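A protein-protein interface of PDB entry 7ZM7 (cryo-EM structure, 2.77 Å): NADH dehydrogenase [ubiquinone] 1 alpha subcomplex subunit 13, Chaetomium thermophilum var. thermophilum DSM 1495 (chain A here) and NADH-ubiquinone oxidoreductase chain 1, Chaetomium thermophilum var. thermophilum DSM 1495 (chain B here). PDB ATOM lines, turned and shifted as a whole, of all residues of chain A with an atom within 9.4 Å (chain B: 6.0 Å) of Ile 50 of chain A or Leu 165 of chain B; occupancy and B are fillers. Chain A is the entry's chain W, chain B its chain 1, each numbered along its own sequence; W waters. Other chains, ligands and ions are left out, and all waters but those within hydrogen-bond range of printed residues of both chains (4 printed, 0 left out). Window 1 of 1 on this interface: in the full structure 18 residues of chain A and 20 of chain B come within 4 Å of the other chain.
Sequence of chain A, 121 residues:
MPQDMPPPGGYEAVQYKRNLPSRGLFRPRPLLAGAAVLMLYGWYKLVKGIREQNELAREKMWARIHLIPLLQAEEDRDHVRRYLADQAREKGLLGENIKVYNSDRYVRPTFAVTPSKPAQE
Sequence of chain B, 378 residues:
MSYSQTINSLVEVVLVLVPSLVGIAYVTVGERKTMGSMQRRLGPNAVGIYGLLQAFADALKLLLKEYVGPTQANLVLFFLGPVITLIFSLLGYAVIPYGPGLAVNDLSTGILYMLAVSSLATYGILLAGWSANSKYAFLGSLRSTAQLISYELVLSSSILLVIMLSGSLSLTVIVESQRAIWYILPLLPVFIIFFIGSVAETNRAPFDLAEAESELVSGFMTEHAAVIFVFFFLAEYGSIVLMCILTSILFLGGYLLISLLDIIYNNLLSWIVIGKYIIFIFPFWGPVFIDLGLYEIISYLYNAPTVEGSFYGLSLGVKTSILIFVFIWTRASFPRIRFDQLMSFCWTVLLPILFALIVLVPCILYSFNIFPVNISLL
The indole nitrogen (NE1) of Trp 43 of chain A lies within hydrogen-bond range of the backbone carbonyl oxygen (O) of Pro 186 of chain B (2.9 Å). N of Val 373 of chain B is in hydrogen-bond range of OD1 of Asn 54 of chain A (3.2 Å). The side-chain amide nitrogen (NE2) of Gln 53 of chain A sits at hydrogen-bond distance from the side-chain hydroxyl (OG) of Ser 177 of chain B (3.5 Å). O of Phe 371 of chain B lies within hydrogen-bond range of ND2 of Asn 54 of chain A, 3.1 Å away.
The backbone NH of Ile 370 of chain B sits at hydrogen-bond distance from the backbone carbonyl oxygen of Leu 365 of chain B, 2.8 Å away. The side-chain hydroxyl of Ser 166 of chain B sits at hydrogen-bond distance from the side-chain hydroxyl of Tyr 183 of chain B (3.3 Å). O of Ile 50 of chain A is in hydrogen-bond range of ND2 of Asn 54 of chain A, 3.2 Å away.
CD1 of Leu 365 of chain B touches CH2 of Trp 43 of chain A, at 3.8 Å. Leu 165 of chain B touches Leu 46 of chain A. Leu 46 of chain A touches Tyr 183 of chain B. Gly 49 of chain A touches Ala 180 of chain B. Ile 50 of chain A touches Leu 165 of chain B (CD1 to O, 3.6 Å). OD1 of Asn 54 of chain A touches CA of Pro 372 of chain B (3.6 Å).
Of the printed residues of chain B, Gly 42 of chain A touches Pro 186 (3.8 Å). Ile 50 of chain A touches three residues of chain B. Of the printed residues of chain A, Leu 165 of chain B touches Leu 46 and Ile 50. No residue of chain A comes within 4 Å of Ser 166 of chain B. Printed residues of chain A within 4 Å of Pro 186 of chain B: Gly 42 (3.8 Å) and Trp 43 (2.9 Å). Of the printed residues of chain A, Asn 369 of chain B touches Arg 51. The nearest residue of chain B that does not touch Ile 50 of chain A is Phe 371 of chain B (4.1 Å). The nearest printed residue of chain A that does not touch Phe 371 of chain B is Ile 50 of chain A (4.1 Å).
Printed residues of chain A that touch a printed residue of chain B: Gly 42, Trp 43, Leu 46, Val 47, Gly 49, Ile 50, Arg 51, Gln 53, Asn 54 and Ala 57. Among the printed residues, 18 pairs touch across the chains. Among the printed residues, no Asp or Glu carboxylate lies within 4 Å of a Lys or Arg side-chain nitrogen of the other chain.
Water W1 bridges O of Asn 369 of chain B and ND2 of Asn 54 of chain A. Water W3 lies within hydrogen-bond range of the backbone carbonyl oxygen of Lys 45 of chain A (3.0 Å) and the backbone carbonyl oxygen of Ala 180 of chain B (3.3 Å). Water W2 bridges NE of Arg 51 of chain A (3.1 Å) and OD1 of Asn 369 of chain B (3.3 Å).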
ATOM      1  N   GLY A  42     -11.753   0.663   5.188  1.00  0.00           N
ATOM      2  CA  GLY A  42     -11.425  -0.175   6.355  1.00  0.00           C
ATOM      3  C   GLY A  42     -10.481   0.538   7.290  1.00  0.00           C
ATOM      4  O   GLY A  42     -10.645   0.397   8.506  1.00  0.00           O
ATOM      5  N   TRP A  43      -9.508   1.258   6.732  1.00  0.00           N
ATOM      6  CA  TRP A  43      -8.529   1.997   7.566  1.00  0.00           C
ATOM      7  C   TRP A  43      -9.217   3.177   8.253  1.00  0.00           C
ATOM      8  O   TRP A  43      -8.766   3.551   9.341  1.00  0.00           O
ATOM      9  CB  TRP A  43      -7.292   2.407   6.762  1.00  0.00           C
ATOM     10  CG  TRP A  43      -6.244   1.341   6.716  1.00  0.00           C
ATOM     11  CD1 TRP A  43      -5.910   0.557   5.650  1.00  0.00           C
ATOM     12  CD2 TRP A  43      -5.394   0.927   7.799  1.00  0.00           C
ATOM     13  NE1 TRP A  43      -4.908  -0.308   5.993  1.00  0.00           N
ATOM     14  CE2 TRP A  43      -4.573  -0.107   7.305  1.00  0.00           C
ATOM     15  CE3 TRP A  43      -5.244   1.330   9.130  1.00  0.00           C
ATOM     16  CZ2 TRP A  43      -3.619  -0.742   8.096  1.00  0.00           C
ATOM     17  CZ3 TRP A  43      -4.301   0.704   9.911  1.00  0.00           C
ATOM     18  CH2 TRP A  43      -3.502  -0.319   9.399  1.00  0.00           C
ATOM     19  N   TYR A  44     -10.289   3.718   7.668  1.00  0.00           N
ATOM     20  CA  TYR A  44     -11.004   4.792   8.394  1.00  0.00           C
ATOM     21  C   TYR A  44     -11.777   4.152   9.546  1.00  0.00           C
ATOM     22  O   TYR A  44     -11.757   4.715  10.644  1.00  0.00           O
ATOM     23  CB  TYR A  44     -11.947   5.530   7.440  1.00  0.00           C
ATOM     24  CG  TYR A  44     -12.995   6.392   8.094  1.00  0.00           C
ATOM     25  CD1 TYR A  44     -12.680   7.643   8.594  1.00  0.00           C
ATOM     26  CD2 TYR A  44     -14.308   5.964   8.195  1.00  0.00           C
ATOM     27  CE1 TYR A  44     -13.639   8.442   9.191  1.00  0.00           C
ATOM     28  CE2 TYR A  44     -15.279   6.749   8.789  1.00  0.00           C
ATOM     29  CZ  TYR A  44     -14.945   7.995   9.288  1.00  0.00           C
ATOM     30  OH  TYR A  44     -15.894   8.779   9.874  1.00  0.00           O
ATOM     31  N   LYS A  45     -12.397   2.999   9.302  1.00  0.00           N
ATOM     32  CA  LYS A  45     -13.232   2.304  10.319  1.00  0.00           C
ATOM     33  C   LYS A  45     -12.363   1.780  11.467  1.00  0.00           C
ATOM     34  O   LYS A  45     -12.804   1.886  12.612  1.00  0.00           O
ATOM     35  CB  LYS A  45     -14.102   1.257   9.617  1.00  0.00           C
ATOM     36  CG  LYS A  45     -14.957   1.785   8.479  1.00  0.00           C
ATOM     37  CD  LYS A  45     -16.023   2.724   8.971  1.00  0.00           C
ATOM     38  CE  LYS A  45     -16.929   2.080   9.998  1.00  0.00           C
ATOM     39  NZ  LYS A  45     -17.681   3.097  10.768  1.00  0.00           N
ATOM     40  N   LEU A  46     -11.187   1.233  11.159  1.00  0.00           N
ATOM     41  CA  LEU A  46     -10.233   0.763  12.195  1.00  0.00           C
ATOM     42  C   LEU A  46      -9.738   1.936  13.038  1.00  0.00           C
ATOM     43  O   LEU A  46      -9.637   1.766  14.254  1.00  0.00           O
ATOM     44  CB  LEU A  46      -9.047   0.103  11.495  1.00  0.00           C
ATOM     45  CG  LEU A  46      -8.136  -0.740  12.383  1.00  0.00           C
ATOM     46  CD1 LEU A  46      -8.877  -1.948  12.935  1.00  0.00           C
ATOM     47  CD2 LEU A  46      -6.906  -1.180  11.615  1.00  0.00           C
ATOM     48  N   VAL A  47      -9.445   3.083  12.424  1.00  0.00           N
ATOM     49  CA  VAL A  47      -8.840   4.221  13.174  1.00  0.00           C
ATOM     50  C   VAL A  47      -9.883   4.806  14.118  1.00  0.00           C
ATOM     51  O   VAL A  47      -9.509   5.359  15.150  1.00  0.00           O
ATOM     52  CB  VAL A  47      -8.198   5.279  12.243  1.00  0.00           C
ATOM     53  CG1 VAL A  47      -8.122   6.671  12.846  1.00  0.00           C
ATOM     54  CG2 VAL A  47      -6.840   4.847  11.719  1.00  0.00           C
ATOM     55  N   LYS A  48     -11.151   4.570  13.833  1.00  0.00           N
ATOM     56  CA  LYS A  48     -12.220   5.076  14.722  1.00  0.00           C
ATOM     57  C   LYS A  48     -12.421   4.069  15.853  1.00  0.00           C
ATOM     58  O   LYS A  48     -12.587   4.502  16.998  1.00  0.00           O
ATOM     59  CB  LYS A  48     -13.525   5.262  13.947  1.00  0.00           C
ATOM     60  CG  LYS A  48     -13.544   6.369  12.910  1.00  0.00           C
ATOM     61  CD  LYS A  48     -14.935   6.906  12.687  1.00  0.00           C
ATOM     62  CE  LYS A  48     -15.534   7.507  13.940  1.00  0.00           C
ATOM     63  NZ  LYS A  48     -16.917   7.988  13.712  1.00  0.00           N
ATOM     64  N   GLY A  49     -12.390   2.778  15.534  1.00  0.00           N
ATOM     65  CA  GLY A  49     -12.625   1.731  16.537  1.00  0.00           C
ATOM     66  C   GLY A  49     -11.547   1.652  17.591  1.00  0.00           C
ATOM     67  O   GLY A  49     -11.885   1.531  18.774  1.00  0.00           O
ATOM     68  N   ILE A  50     -10.283   1.697  17.188  1.00  0.00           N
ATOM     69  CA  ILE A  50      -9.219   1.498  18.203  1.00  0.00           C
ATOM     70  C   ILE A  50      -9.129   2.761  19.068  1.00  0.00           C
ATOM     71  O   ILE A  50      -8.633   2.673  20.182  1.00  0.00           O
ATOM     72  CB  ILE A  50      -7.894   1.133  17.506  1.00  0.00           C
ATOM     73  CG1 ILE A  50      -8.053  -0.088  16.601  1.00  0.00           C
ATOM     74  CG2 ILE A  50      -6.780   0.924  18.518  1.00  0.00           C
ATOM     75  CD1 ILE A  50      -6.766  -0.528  15.946  1.00  0.00           C
ATOM     76  N   ARG A  51      -9.632   3.889  18.577  1.00  0.00           N
ATOM     77  CA  ARG A  51      -9.676   5.120  19.403  1.00  0.00           C
ATOM     78  C   ARG A  51     -10.728   4.891  20.490  1.00  0.00           C
ATOM     79  O   ARG A  51     -10.440   5.154  21.664  1.00  0.00           O
ATOM     80  CB  ARG A  51      -9.759   6.351  18.501  1.00  0.00           C
ATOM     81  CG  ARG A  51      -8.430   6.769  17.891  1.00  0.00           C
ATOM     82  CD  ARG A  51      -8.359   8.274  17.744  1.00  0.00           C
ATOM     83  NE  ARG A  51      -7.089   8.753  17.222  1.00  0.00           N
ATOM     84  CZ  ARG A  51      -6.922   9.264  16.009  1.00  0.00           C
ATOM     85  NH1 ARG A  51      -5.730   9.684  15.625  1.00  0.00           N
ATOM     86  NH2 ARG A  51      -7.952   9.373  15.191  1.00  0.00           N
ATOM     87  N   GLU A  52     -11.914   4.426  20.086  1.00  0.00           N
ATOM     88  CA  GLU A  52     -13.010   4.110  21.041  1.00  0.00           C
ATOM     89  C   GLU A  52     -12.580   3.000  22.004  1.00  0.00           C
ATOM     90  O   GLU A  52     -12.907   3.113  23.194  1.00  0.00           O
ATOM     91  CB  GLU A  52     -14.281   3.732  20.279  1.00  0.00           C
ATOM     92  CG  GLU A  52     -15.377   3.131  21.138  1.00  0.00           C
ATOM     93  CD  GLU A  52     -16.793   3.503  20.732  1.00  0.00           C
ATOM     94  OE1 GLU A  52     -16.970   4.552  20.076  1.00  0.00           O
ATOM     95  OE2 GLU A  52     -17.719   2.746  21.078  1.00  0.00           O
ATOM     96  N   GLN A  53     -11.860   1.992  21.521  1.00  0.00           N
ATOM     97  CA  GLN A  53     -11.407   0.888  22.396  1.00  0.00           C
ATOM     98  C   GLN A  53     -10.512   1.468  23.482  1.00  0.00           C
ATOM     99  O   GLN A  53     -10.689   1.109  24.644  1.00  0.00           O
ATOM    100  CB  GLN A  53     -10.543  -0.100  21.619  1.00  0.00           C
ATOM    101  CG  GLN A  53     -11.117  -1.500  21.530  1.00  0.00           C
ATOM    102  CD  GLN A  53     -10.223  -2.367  20.680  1.00  0.00           C
ATOM    103  OE1 GLN A  53      -9.063  -2.045  20.449  1.00  0.00           O
ATOM    104  NE2 GLN A  53     -10.758  -3.480  20.210  1.00  0.00           N
ATOM    105  N   ASN A  54      -9.611   2.364  23.112  1.00  0.00           N
ATOM    106  CA  ASN A  54      -8.657   2.975  24.067  1.00  0.00           C
ATOM    107  C   ASN A  54      -9.421   3.792  25.110  1.00  0.00           C
ATOM    108  O   ASN A  54      -9.001   3.791  26.265  1.00  0.00           O
ATOM    109  CB  ASN A  54      -7.582   3.736  23.298  1.00  0.00           C
ATOM    110  CG  ASN A  54      -6.560   2.830  22.650  1.00  0.00           C
ATOM    111  OD1 ASN A  54      -6.394   1.686  23.056  1.00  0.00           O
ATOM    112  ND2 ASN A  54      -5.857   3.333  21.649  1.00  0.00           N
ATOM    113  N   GLU A  55     -10.469   4.493  24.696  1.00  0.00           N
ATOM    114  CA  GLU A  55     -11.324   5.281  25.620  1.00  0.00           C
ATOM    115  C   GLU A  55     -12.132   4.366  26.552  1.00  0.00           C
ATOM    116  O   GLU A  55     -12.347   4.746  27.714  1.00  0.00           O
ATOM    117  CB  GLU A  55     -12.093   6.334  24.820  1.00  0.00           C
ATOM    118  CG  GLU A  55     -11.195   7.406  24.242  1.00  0.00           C
ATOM    119  CD  GLU A  55     -10.057   7.821  25.159  1.00  0.00           C
ATOM    120  OE1 GLU A  55     -10.327   8.137  26.337  1.00  0.00           O
ATOM    121  OE2 GLU A  55      -8.901   7.823  24.695  1.00  0.00           O
ATOM    122  N   LEU A  56     -12.596   3.221  26.055  1.00  0.00           N
ATOM    123  CA  LEU A  56     -13.290   2.238  26.927  1.00  0.00           C
ATOM    124  C   LEU A  56     -12.304   1.726  27.973  1.00  0.00           C
ATOM    125  O   LEU A  56     -12.716   1.520  29.117  1.00  0.00           O
ATOM    126  CB  LEU A  56     -13.869   1.107  26.074  1.00  0.00           C
ATOM    127  CG  LEU A  56     -15.047   1.491  25.186  1.00  0.00           C
ATOM    128  CD1 LEU A  56     -15.403   0.353  24.245  1.00  0.00           C
ATOM    129  CD2 LEU A  56     -16.242   1.894  26.028  1.00  0.00           C
ATOM    130  N   ALA A  57     -11.051   1.526  27.587  1.00  0.00           N
ATOM    131  CA  ALA A  57     -10.006   1.105  28.542  1.00  0.00           C
ATOM    132  C   ALA A  57      -9.747   2.167  29.624  1.00  0.00           C
ATOM    133  O   ALA A  57      -9.503   1.775  30.766  1.00  0.00           O
ATOM    134  CB  ALA A  57      -8.760   0.683  27.812  1.00  0.00           C
ATOM    135  N   ARG A  58      -9.789   3.453  29.286  1.00  0.00           N
ATOM    136  CA  ARG A  58      -9.611   4.511  30.311  1.00  0.00           C
ATOM    137  C   ARG A  58     -10.718   4.408  31.362  1.00  0.00           C
ATOM    138  O   ARG A  58     -10.399   4.540  32.549  1.00  0.00           O
ATOM    139  CB  ARG A  58      -9.559   5.895  29.669  1.00  0.00           C
ATOM    140  CG  ARG A  58      -9.101   6.996  30.612  1.00  0.00           C
ATOM    141  CD  ARG A  58      -9.212   8.371  29.987  1.00  0.00           C
ATOM    142  NE  ARG A  58      -8.643   8.384  28.652  1.00  0.00           N
ATOM    143  CZ  ARG A  58      -7.370   8.625  28.375  1.00  0.00           C
ATOM    144  NH1 ARG A  58      -6.957   8.608  27.121  1.00  0.00           N
ATOM    145  NH2 ARG A  58      -6.515   8.877  29.348  1.00  0.00           N
ATOM    146  N   LEU B 160       1.072 -12.249  12.498  1.00  0.00           N
ATOM    147  CA  LEU B 160       1.660 -11.155  13.258  1.00  0.00           C
ATOM    148  C   LEU B 160       0.972  -9.838  12.953  1.00  0.00           C
ATOM    149  O   LEU B 160       0.775  -9.013  13.845  1.00  0.00           O
ATOM    150  CB  LEU B 160       3.157 -11.068  12.937  1.00  0.00           C
ATOM    151  CG  LEU B 160       4.081 -10.153  13.732  1.00  0.00           C
ATOM    152  CD1 LEU B 160       4.193 -10.598  15.161  1.00  0.00           C
ATOM    153  CD2 LEU B 160       5.429 -10.131  13.101  1.00  0.00           C
ATOM    154  N   LEU B 161       0.589  -9.628  11.698  1.00  0.00           N
ATOM    155  CA  LEU B 161       0.002  -8.353  11.306  1.00  0.00           C
ATOM    156  C   LEU B 161      -1.396  -8.164  11.877  1.00  0.00           C
ATOM    157  O   LEU B 161      -1.833  -7.029  12.065  1.00  0.00           O
ATOM    158  CB  LEU B 161      -0.016  -8.241   9.783  1.00  0.00           C
ATOM    159  CG  LEU B 161       1.349  -8.051   9.134  1.00  0.00           C
ATOM    160  CD1 LEU B 161       1.356  -8.582   7.716  1.00  0.00           C
ATOM    161  CD2 LEU B 161       1.753  -6.586   9.193  1.00  0.00           C
ATOM    162  N   VAL B 162      -2.122  -9.254  12.121  1.00  0.00           N
ATOM    163  CA  VAL B 162      -3.418  -9.155  12.779  1.00  0.00           C
ATOM    164  C   VAL B 162      -3.247  -8.838  14.257  1.00  0.00           C
ATOM    165  O   VAL B 162      -3.999  -8.040  14.820  1.00  0.00           O
ATOM    166  CB  VAL B 162      -4.227 -10.448  12.555  1.00  0.00           C
ATOM    167  CG1 VAL B 162      -5.308 -10.602  13.599  1.00  0.00           C
ATOM    168  CG2 VAL B 162      -4.833 -10.463  11.155  1.00  0.00           C
ATOM    169  N   ILE B 163      -2.247  -9.444  14.902  1.00  0.00           N
ATOM    170  CA  ILE B 163      -2.017  -9.230  16.328  1.00  0.00           C
ATOM    171  C   ILE B 163      -1.699  -7.774  16.611  1.00  0.00           C
ATOM    172  O   ILE B 163      -2.084  -7.240  17.655  1.00  0.00           O
ATOM    173  CB  ILE B 163      -0.895 -10.158  16.828  1.00  0.00           C
ATOM    174  CG1 ILE B 163      -1.190 -11.611  16.459  1.00  0.00           C
ATOM    175  CG2 ILE B 163      -0.683 -10.005  18.330  1.00  0.00           C
ATOM    176  CD1 ILE B 163      -2.400 -12.192  17.113  1.00  0.00           C
ATOM    177  N   MET B 164      -0.961  -7.129  15.705  1.00  0.00           N
ATOM    178  CA  MET B 164      -0.647  -5.683  15.853  1.00  0.00           C
ATOM    179  C   MET B 164      -1.949  -4.885  15.949  1.00  0.00           C
ATOM    180  O   MET B 164      -2.025  -4.002  16.815  1.00  0.00           O
ATOM    181  CB  MET B 164       0.176  -5.200  14.658  1.00  0.00           C
ATOM    182  CG  MET B 164       1.530  -5.872  14.555  1.00  0.00           C
ATOM    183  SD  MET B 164       2.503  -5.283  13.155  1.00  0.00           S
ATOM    184  CE  MET B 164       4.035  -6.176  13.414  1.00  0.00           C
ATOM    185  N   LEU B 165      -2.924  -5.169  15.088  1.00  0.00           N
ATOM    186  CA  LEU B 165      -4.240  -4.472  15.098  1.00  0.00           C
ATOM    187  C   LEU B 165      -5.071  -4.786  16.344  1.00  0.00           C
ATOM    188  O   LEU B 165      -5.685  -3.852  16.876  1.00  0.00           O
ATOM    189  CB  LEU B 165      -5.012  -4.933  13.860  1.00  0.00           C
ATOM    190  CG  LEU B 165      -5.000  -4.004  12.656  1.00  0.00           C
ATOM    191  CD1 LEU B 165      -3.615  -3.926  12.036  1.00  0.00           C
ATOM    192  CD2 LEU B 165      -6.008  -4.507  11.644  1.00  0.00           C
ATOM    193  N   SER B 166      -5.099  -6.048  16.782  1.00  0.00           N
ATOM    194  CA  SER B 166      -5.957  -6.467  17.924  1.00  0.00           C
ATOM    195  C   SER B 166      -5.270  -6.184  19.261  1.00  0.00           C
ATOM    196  O   SER B 166      -5.969  -5.766  20.196  1.00  0.00           O
ATOM    197  CB  SER B 166      -6.309  -7.930  17.809  1.00  0.00           C
ATOM    198  OG  SER B 166      -6.648  -8.272  16.477  1.00  0.00           O
ATOM    199  N   GLY B 167      -3.968  -6.445  19.361  1.00  0.00           N
ATOM    200  CA  GLY B 167      -3.225  -6.244  20.619  1.00  0.00           C
ATOM    201  C   GLY B 167      -3.152  -7.498  21.466  1.00  0.00           C
ATOM    202  O   GLY B 167      -2.480  -7.444  22.504  1.00  0.00           O
ATOM    203  N   SER B 177     -12.596  -7.501  18.482  1.00  0.00           N
ATOM    204  CA  SER B 177     -11.936  -6.275  17.975  1.00  0.00           C
ATOM    205  C   SER B 177     -12.441  -5.949  16.572  1.00  0.00           C
ATOM    206  O   SER B 177     -12.303  -4.793  16.151  1.00  0.00           O
ATOM    207  CB  SER B 177     -10.451  -6.486  17.985  1.00  0.00           C
ATOM    208  OG  SER B 177      -9.984  -6.733  19.301  1.00  0.00           O
ATOM    209  N   ALA B 180     -15.586  -3.278  15.217  1.00  0.00           N
ATOM    210  CA  ALA B 180     -15.339  -2.018  14.475  1.00  0.00           C
ATOM    211  C   ALA B 180     -15.296  -2.246  12.960  1.00  0.00           C
ATOM    212  O   ALA B 180     -15.931  -1.470  12.239  1.00  0.00           O
ATOM    213  CB  ALA B 180     -14.024  -1.445  14.928  1.00  0.00           C
ATOM    214  N   TYR B 183     -11.171  -7.511   9.377  1.00  0.00           N
ATOM    215  CA  TYR B 183      -9.786  -7.251   9.020  1.00  0.00           C
ATOM    216  C   TYR B 183      -9.491  -7.482   7.552  1.00  0.00           C
ATOM    217  O   TYR B 183      -8.422  -7.085   7.091  1.00  0.00           O
ATOM    218  CB  TYR B 183      -8.860  -8.091   9.879  1.00  0.00           C
ATOM    219  CG  TYR B 183      -8.739  -7.535  11.262  1.00  0.00           C
ATOM    220  CD1 TYR B 183      -9.258  -6.291  11.565  1.00  0.00           C
ATOM    221  CD2 TYR B 183      -8.133  -8.256  12.274  1.00  0.00           C
ATOM    222  CE1 TYR B 183      -9.168  -5.778  12.823  1.00  0.00           C
ATOM    223  CE2 TYR B 183      -8.037  -7.746  13.541  1.00  0.00           C
ATOM    224  CZ  TYR B 183      -8.558  -6.500  13.807  1.00  0.00           C
ATOM    225  OH  TYR B 183      -8.473  -5.970  15.058  1.00  0.00           O
ATOM    226  N   PRO B 186      -9.146  -3.515   5.926  1.00  0.00           N
ATOM    227  CA  PRO B 186      -7.905  -2.750   5.977  1.00  0.00           C
ATOM    228  C   PRO B 186      -6.652  -3.589   5.681  1.00  0.00           C
ATOM    229  O   PRO B 186      -5.694  -3.029   5.208  1.00  0.00           O
ATOM    230  CB  PRO B 186      -7.869  -2.267   7.434  1.00  0.00           C
ATOM    231  CG  PRO B 186      -8.602  -3.330   8.211  1.00  0.00           C
ATOM    232  CD  PRO B 186      -9.667  -3.828   7.260  1.00  0.00           C
ATOM    233  N   LEU B 187      -6.685  -4.898   5.933  1.00  0.00           N
ATOM    234  CA  LEU B 187      -5.538  -5.752   5.635  1.00  0.00           C
ATOM    235  C   LEU B 187      -5.848  -6.685   4.489  1.00  0.00           C
ATOM    236  O   LEU B 187      -5.636  -7.892   4.584  1.00  0.00           O
ATOM    237  CB  LEU B 187      -5.077  -6.521   6.872  1.00  0.00           C
ATOM    238  CG  LEU B 187      -4.238  -5.678   7.828  1.00  0.00           C
ATOM    239  CD1 LEU B 187      -5.031  -4.646   8.536  1.00  0.00           C
ATOM    240  CD2 LEU B 187      -3.590  -6.581   8.842  1.00  0.00           C
ATOM    241  N   VAL B 361       2.904  -1.352   8.765  1.00  0.00           N
ATOM    242  CA  VAL B 361       1.690  -1.356   9.583  1.00  0.00           C
ATOM    243  C   VAL B 361       1.895  -0.706  10.945  1.00  0.00           C
ATOM    244  O   VAL B 361       1.176   0.254  11.255  1.00  0.00           O
ATOM    245  CB  VAL B 361       1.109  -2.781   9.662  1.00  0.00           C
ATOM    246  CG1 VAL B 361       0.008  -2.863  10.672  1.00  0.00           C
ATOM    247  CG2 VAL B 361       0.542  -3.141   8.319  1.00  0.00           C
ATOM    248  N   LEU B 365       0.007   2.773  12.521  1.00  0.00           N
ATOM    249  CA  LEU B 365      -0.654   2.749  13.822  1.00  0.00           C
ATOM    250  C   LEU B 365      -0.036   3.733  14.800  1.00  0.00           C
ATOM    251  O   LEU B 365      -0.727   4.249  15.683  1.00  0.00           O
ATOM    252  CB  LEU B 365      -0.643   1.340  14.403  1.00  0.00           C
ATOM    253  CG  LEU B 365      -1.634   0.292  13.919  1.00  0.00           C
ATOM    254  CD1 LEU B 365      -1.400  -0.215  12.537  1.00  0.00           C
ATOM    255  CD2 LEU B 365      -1.501  -0.867  14.875  1.00  0.00           C
ATOM    256  N   ASN B 369      -2.120   7.469  16.131  1.00  0.00           N
ATOM    257  CA  ASN B 369      -2.404   7.209  17.576  1.00  0.00           C
ATOM    258  C   ASN B 369      -3.355   6.020  17.715  1.00  0.00           C
ATOM    259  O   ASN B 369      -4.372   6.165  18.398  1.00  0.00           O
ATOM    260  CB  ASN B 369      -2.872   8.470  18.309  1.00  0.00           C
ATOM    261  CG  ASN B 369      -2.692   8.390  19.807  1.00  0.00           C
ATOM    262  OD1 ASN B 369      -3.567   8.802  20.560  1.00  0.00           O
ATOM    263  ND2 ASN B 369      -1.572   7.842  20.248  1.00  0.00           N
ATOM    264  N   ILE B 370      -3.057   4.892  17.068  1.00  0.00           N
ATOM    265  CA  ILE B 370      -4.044   3.770  17.043  1.00  0.00           C
ATOM    266  C   ILE B 370      -3.457   2.474  17.561  1.00  0.00           C
ATOM    267  O   ILE B 370      -3.956   1.424  17.157  1.00  0.00           O
ATOM    268  CB  ILE B 370      -4.806   3.611  15.710  1.00  0.00           C
ATOM    269  CG1 ILE B 370      -3.903   3.676  14.479  1.00  0.00           C
ATOM    270  CG2 ILE B 370      -5.941   4.617  15.627  1.00  0.00           C
ATOM    271  CD1 ILE B 370      -4.393   2.833  13.333  1.00  0.00           C
ATOM    272  N   PHE B 371      -2.393   2.564  18.360  1.00  0.00           N
ATOM    273  CA  PHE B 371      -1.871   1.346  19.020  1.00  0.00           C
ATOM    274  C   PHE B 371      -2.942   0.940  20.046  1.00  0.00           C
ATOM    275  O   PHE B 371      -3.285   1.796  20.870  1.00  0.00           O
ATOM    276  CB  PHE B 371      -0.514   1.592  19.685  1.00  0.00           C
ATOM    277  CG  PHE B 371       0.695   1.493  18.788  1.00  0.00           C
ATOM    278  CD1 PHE B 371       0.722   0.614  17.719  1.00  0.00           C
ATOM    279  CD2 PHE B 371       1.821   2.260  19.036  1.00  0.00           C
ATOM    280  CE1 PHE B 371       1.841   0.520  16.907  1.00  0.00           C
ATOM    281  CE2 PHE B 371       2.939   2.165  18.224  1.00  0.00           C
ATOM    282  CZ  PHE B 371       2.946   1.295  17.160  1.00  0.00           C
ATOM    283  N   PRO B 372      -3.525  -0.282  20.035  1.00  0.00           N
ATOM    284  CA  PRO B 372      -4.489  -0.683  21.061  1.00  0.00           C
ATOM    285  C   PRO B 372      -3.809  -0.942  22.393  1.00  0.00           C
ATOM    286  O   PRO B 372      -2.599  -1.142  22.477  1.00  0.00           O
ATOM    287  CB  PRO B 372      -5.102  -1.964  20.490  1.00  0.00           C
ATOM    288  CG  PRO B 372      -4.048  -2.509  19.645  1.00  0.00           C
ATOM    289  CD  PRO B 372      -3.284  -1.362  19.067  1.00  0.00           C
ATOM    290  N   VAL B 373      -4.640  -0.947  23.427  1.00  0.00           N
ATOM    291  CA  VAL B 373      -4.153  -1.263  24.794  1.00  0.00           C
ATOM    292  C   VAL B 373      -4.027  -2.788  24.886  1.00  0.00           C
ATOM    293  O   VAL B 373      -4.855  -3.488  24.289  1.00  0.00           O
ATOM    294  CB  VAL B 373      -5.104  -0.650  25.831  1.00  0.00           C
ATOM    295  CG1 VAL B 373      -4.782   0.806  26.098  1.00  0.00           C
ATOM    296  CG2 VAL B 373      -6.555  -0.805  25.408  1.00  0.00           C
HETATM  297  O   HOH W   1      -6.101   6.258  20.749  1.00  0.00           O
HETATM  298  O   HOH W   2      -6.399  10.403  19.775  1.00  0.00           O
HETATM  299  O   HOH W   3     -15.637   1.480  13.581  1.00  0.00           O
HETATM  300  O   HOH W   4      -2.807   4.703  21.464  1.00  0.00           O
